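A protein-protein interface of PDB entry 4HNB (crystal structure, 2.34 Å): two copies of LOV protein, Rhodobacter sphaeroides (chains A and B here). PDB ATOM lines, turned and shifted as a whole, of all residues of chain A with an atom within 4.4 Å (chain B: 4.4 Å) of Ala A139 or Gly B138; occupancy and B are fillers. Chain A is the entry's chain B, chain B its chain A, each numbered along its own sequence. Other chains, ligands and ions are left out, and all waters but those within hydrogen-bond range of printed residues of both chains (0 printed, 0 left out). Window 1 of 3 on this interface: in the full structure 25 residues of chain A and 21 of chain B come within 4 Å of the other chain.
Val A19 touches Arg B159 (CG1 to NH1, 3.5 Å). Ala B134 touches Gly A135 (O to CA, 3.2 Å). Gly A135 touches Gly B138. O of Gly A135 touches CD of Arg B159, at 3.3 Å. CA of His A136 touches NE of Arg B159, at 3.9 Å. Gly A138 touches Gly B135. C of Gly A138 touches N of Ala B139, at 3.6 Å. Ala A139 touches Gly B138 (N to C, 3.6 Å). Ala B139 touches Ala A139. Arg B159 touches Ala A139.
Of the printed residues of chain B, Val A19 touches Arg B159. Of the printed residues of chain B, His A136 touches Arg B159. Of chain B, only Gly B138, Ala B139 and Arg B159 come within 4 Å of Ala A139. Of the printed residues of chain A, Gly B135 touches Gly A138 (3.4 Å). Of the printed residues of chain A, Gly B138 touches Gly A135 (3.2 Å) and Ala A139 (3.6 Å). The nearest printed residue of chain A that does not touch Gly B138 is Gly A138 (4.002 Å).
Of the 10 printed residues of chain B, 5 touch a printed residue of chain A. Hydrophobic or aromatic side chains of chain B within 4 Å of the printed part of chain A: Ala B139. Hydrophobic or aromatic side chains of chain A that line the printed part of chain B: Val A19 and Ala A139.
Gly A135 touches Gly B138, and with the chains exchanged Gly A138 touches Gly B135. Gly A138 touches Ala B139, and with the chains exchanged Ala A139 touches Gly B138. Ala B139 touches its own counterpart, Ala A139.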
ATOM      1  N   VAL A  19     -18.646   4.772 -15.524  1.00  0.00           N
ATOM      2  CA  VAL A  19     -19.516   4.571 -14.366  1.00  0.00           C
ATOM      3  C   VAL A  19     -19.796   5.875 -13.628  1.00  0.00           C
ATOM      4  O   VAL A  19     -19.000   6.823 -13.691  1.00  0.00           O
ATOM      5  CB  VAL A  19     -18.961   3.526 -13.367  1.00  0.00           C
ATOM      6  CG1 VAL A  19     -18.978   2.148 -13.994  1.00  0.00           C
ATOM      7  CG2 VAL A  19     -17.567   3.915 -12.866  1.00  0.00           C
ATOM      8  N   GLY A 135     -19.646  -6.414 -13.006  1.00  0.00           N
ATOM      9  CA  GLY A 135     -19.038  -5.677 -14.096  1.00  0.00           C
ATOM     10  C   GLY A 135     -18.749  -4.237 -13.694  1.00  0.00           C
ATOM     11  O   GLY A 135     -17.676  -3.692 -13.979  1.00  0.00           O
ATOM     12  N   HIS A 136     -19.711  -3.623 -13.010  1.00  0.00           N
ATOM     13  CA  HIS A 136     -19.570  -2.253 -12.554  1.00  0.00           C
ATOM     14  C   HIS A 136     -18.409  -2.167 -11.571  1.00  0.00           C
ATOM     15  O   HIS A 136     -17.573  -1.264 -11.651  1.00  0.00           O
ATOM     16  CB  HIS A 136     -20.871  -1.773 -11.888  1.00  0.00           C
ATOM     17  CG  HIS A 136     -20.795  -0.380 -11.351  1.00  0.00           C
ATOM     18  ND1 HIS A 136     -21.457   0.679 -11.927  1.00  0.00           N
ATOM     19  CD2 HIS A 136     -20.119   0.135 -10.288  1.00  0.00           C
ATOM     20  CE1 HIS A 136     -21.199   1.787 -11.251  1.00  0.00           C
ATOM     21  NE2 HIS A 136     -20.386   1.478 -10.250  1.00  0.00           N
ATOM     22  N   ALA A 137     -18.369  -3.120 -10.648  1.00  0.00           N
ATOM     23  CA  ALA A 137     -17.307  -3.181  -9.647  1.00  0.00           C
ATOM     24  C   ALA A 137     -15.934  -3.178 -10.307  1.00  0.00           C
ATOM     25  O   ALA A 137     -15.014  -2.506  -9.826  1.00  0.00           O
ATOM     26  CB  ALA A 137     -17.468  -4.397  -8.774  1.00  0.00           C
ATOM     27  N   GLY A 138     -15.812  -3.918 -11.412  1.00  0.00           N
ATOM     28  CA  GLY A 138     -14.566  -4.011 -12.161  1.00  0.00           C
ATOM     29  C   GLY A 138     -14.130  -2.717 -12.833  1.00  0.00           C
ATOM     30  O   GLY A 138     -12.961  -2.328 -12.750  1.00  0.00           O
ATOM     31  N   ALA A 139     -15.067  -2.047 -13.499  1.00  0.00           N
ATOM     32  CA  ALA A 139     -14.803  -0.739 -14.080  1.00  0.00           C
ATOM     33  C   ALA A 139     -14.429   0.268 -12.993  1.00  0.00           C
ATOM     34  O   ALA A 139     -13.545   1.101 -13.193  1.00  0.00           O
ATOM     35  CB  ALA A 139     -15.999  -0.269 -14.827  1.00  0.00           C
ATOM     36  N   LEU A 140     -15.113   0.209 -11.852  1.00  0.00           N
ATOM     37  CA  LEU A 140     -14.795   1.095 -10.725  1.00  0.00           C
ATOM     38  C   LEU A 140     -13.334   0.939 -10.270  1.00  0.00           C
ATOM     39  O   LEU A 140     -12.561   1.908 -10.268  1.00  0.00           O
ATOM     40  CB  LEU A 140     -15.744   0.853  -9.543  1.00  0.00           C
ATOM     41  CG  LEU A 140     -15.530   1.761  -8.319  1.00  0.00           C
ATOM     42  CD1 LEU A 140     -15.715   3.216  -8.693  1.00  0.00           C
ATOM     43  CD2 LEU A 140     -16.468   1.420  -7.173  1.00  0.00           C
ATOM     44  N   THR A 141     -12.950  -0.283  -9.911  1.00  0.00           N
ATOM     45  CA  THR A 141     -11.597  -0.558  -9.445  1.00  0.00           C
ATOM     46  C   THR A 141     -10.550  -0.032 -10.417  1.00  0.00           C
ATOM     47  O   THR A 141      -9.523   0.499 -10.011  1.00  0.00           O
ATOM     48  CB  THR A 141     -11.391  -2.054  -9.276  1.00  0.00           C
ATOM     49  OG1 THR A 141     -12.432  -2.563  -8.438  1.00  0.00           O
ATOM     50  CG2 THR A 141     -10.017  -2.351  -8.661  1.00  0.00           C
ATOM     51  N   GLY A 142     -10.822  -0.169 -11.707  1.00  0.00           N
ATOM     52  CA  GLY A 142      -9.963   0.435 -12.708  1.00  0.00           C
ATOM     53  C   GLY A 142      -9.816   1.939 -12.539  1.00  0.00           C
ATOM     54  O   GLY A 142      -8.734   2.489 -12.722  1.00  0.00           O
ATOM     55  N   GLU A 143     -10.910   2.609 -12.193  1.00  0.00           N
ATOM     56  CA  GLU A 143     -10.902   4.050 -11.986  1.00  0.00           C
ATOM     57  C   GLU A 143     -10.133   4.362 -10.698  1.00  0.00           C
ATOM     58  O   GLU A 143      -9.399   5.346 -10.607  1.00  0.00           O
ATOM     59  CB  GLU A 143     -12.346   4.541 -11.849  1.00  0.00           C
ATOM     60  CG  GLU A 143     -12.930   5.401 -12.964  1.00  0.00           C
ATOM     61  CD  GLU A 143     -12.521   5.026 -14.369  1.00  0.00           C
ATOM     62  OE1 GLU A 143     -11.336   5.197 -14.713  1.00  0.00           O
ATOM     63  OE2 GLU A 143     -13.391   4.599 -15.150  1.00  0.00           O
ATOM     64  N   ALA B 134     -17.140 -11.465 -14.391  1.00  0.00           N
ATOM     65  CA  ALA B 134     -17.912 -10.268 -14.691  1.00  0.00           C
ATOM     66  C   ALA B 134     -17.132  -9.016 -14.306  1.00  0.00           C
ATOM     67  O   ALA B 134     -17.121  -8.043 -15.048  1.00  0.00           O
ATOM     68  CB  ALA B 134     -19.238 -10.316 -13.975  1.00  0.00           C
ATOM     69  N   GLY B 135     -16.463  -9.053 -13.157  1.00  0.00           N
ATOM     70  CA  GLY B 135     -15.543  -7.992 -12.779  1.00  0.00           C
ATOM     71  C   GLY B 135     -14.464  -7.760 -13.819  1.00  0.00           C
ATOM     72  O   GLY B 135     -14.259  -6.626 -14.264  1.00  0.00           O
ATOM     73  N   HIS B 136     -13.787  -8.841 -14.219  1.00  0.00           N
ATOM     74  CA  HIS B 136     -12.752  -8.776 -15.253  1.00  0.00           C
ATOM     75  C   HIS B 136     -13.285  -8.105 -16.509  1.00  0.00           C
ATOM     76  O   HIS B 136     -12.706  -7.132 -16.987  1.00  0.00           O
ATOM     77  CB  HIS B 136     -12.211 -10.171 -15.575  1.00  0.00           C
ATOM     78  CG  HIS B 136     -11.085 -10.170 -16.583  1.00  0.00           C
ATOM     79  ND1 HIS B 136      -9.815 -10.582 -16.258  1.00  0.00           N
ATOM     80  CD2 HIS B 136     -11.064  -9.797 -17.874  1.00  0.00           C
ATOM     81  CE1 HIS B 136      -9.044 -10.472 -17.336  1.00  0.00           C
ATOM     82  NE2 HIS B 136      -9.767 -10.000 -18.324  1.00  0.00           N
ATOM     83  N   ALA B 137     -14.402  -8.609 -17.027  1.00  0.00           N
ATOM     84  CA  ALA B 137     -15.060  -7.995 -18.182  1.00  0.00           C
ATOM     85  C   ALA B 137     -15.308  -6.492 -18.000  1.00  0.00           C
ATOM     86  O   ALA B 137     -15.143  -5.706 -18.941  1.00  0.00           O
ATOM     87  CB  ALA B 137     -16.378  -8.714 -18.485  1.00  0.00           C
ATOM     88  N   GLY B 138     -15.715  -6.094 -16.796  1.00  0.00           N
ATOM     89  CA  GLY B 138     -15.951  -4.688 -16.500  1.00  0.00           C
ATOM     90  C   GLY B 138     -14.685  -3.856 -16.629  1.00  0.00           C
ATOM     91  O   GLY B 138     -14.678  -2.802 -17.285  1.00  0.00           O
ATOM     92  N   ALA B 139     -13.606  -4.340 -16.007  1.00  0.00           N
ATOM     93  CA  ALA B 139     -12.294  -3.702 -16.124  1.00  0.00           C
ATOM     94  C   ALA B 139     -11.826  -3.647 -17.579  1.00  0.00           C
ATOM     95  O   ALA B 139     -11.408  -2.590 -18.052  1.00  0.00           O
ATOM     96  CB  ALA B 139     -11.275  -4.415 -15.258  1.00  0.00           C
ATOM     97  N   LEU B 140     -11.911  -4.773 -18.290  1.00  0.00           N
ATOM     98  CA  LEU B 140     -11.527  -4.823 -19.709  1.00  0.00           C
ATOM     99  C   LEU B 140     -12.217  -3.718 -20.511  1.00  0.00           C
ATOM    100  O   LEU B 140     -11.572  -2.937 -21.219  1.00  0.00           O
ATOM    101  CB  LEU B 140     -11.927  -6.160 -20.317  1.00  0.00           C
ATOM    102  CG  LEU B 140     -11.092  -6.758 -21.451  1.00  0.00           C
ATOM    103  CD1 LEU B 140     -11.934  -7.694 -22.293  1.00  0.00           C
ATOM    104  CD2 LEU B 140     -10.401  -5.732 -22.321  1.00  0.00           C
ATOM    105  N   THR B 141     -13.538  -3.683 -20.408  1.00  0.00           N
ATOM    106  CA  THR B 141     -14.337  -2.745 -21.176  1.00  0.00           C
ATOM    107  C   THR B 141     -13.824  -1.329 -20.962  1.00  0.00           C
ATOM    108  O   THR B 141     -13.753  -0.539 -21.899  1.00  0.00           O
ATOM    109  CB  THR B 141     -15.825  -2.845 -20.793  1.00  0.00           C
ATOM    110  OG1 THR B 141     -16.303  -4.167 -21.081  1.00  0.00           O
ATOM    111  CG2 THR B 141     -16.641  -1.834 -21.573  1.00  0.00           C
ATOM    112  N   GLY B 142     -13.446  -1.026 -19.724  1.00  0.00           N
ATOM    113  CA  GLY B 142     -12.832   0.246 -19.412  1.00  0.00           C
ATOM    114  C   GLY B 142     -11.567   0.463 -20.217  1.00  0.00           C
ATOM    115  O   GLY B 142     -11.353   1.540 -20.762  1.00  0.00           O
ATOM    116  N   ARG B 159     -20.303  -2.910 -21.368  1.00  0.00           N
ATOM    117  CA  ARG B 159     -19.834  -3.560 -20.145  1.00  0.00           C
ATOM    118  C   ARG B 159     -20.804  -4.638 -19.663  1.00  0.00           C
ATOM    119  O   ARG B 159     -20.396  -5.775 -19.390  1.00  0.00           O
ATOM    120  CB  ARG B 159     -19.590  -2.541 -19.025  1.00  0.00           C
ATOM    121  CG  ARG B 159     -19.213  -3.192 -17.694  1.00  0.00           C
ATOM    122  CD  ARG B 159     -18.877  -2.182 -16.613  1.00  0.00           C
ATOM    123  NE  ARG B 159     -19.972  -1.250 -16.336  1.00  0.00           N
ATOM    124  CZ  ARG B 159     -20.015   0.003 -16.777  1.00  0.00           C
ATOM    125  NH1 ARG B 159     -21.052   0.782 -16.475  1.00  0.00           N
ATOM    126  NH2 ARG B 159     -19.026   0.478 -17.527  1.00  0.00           N
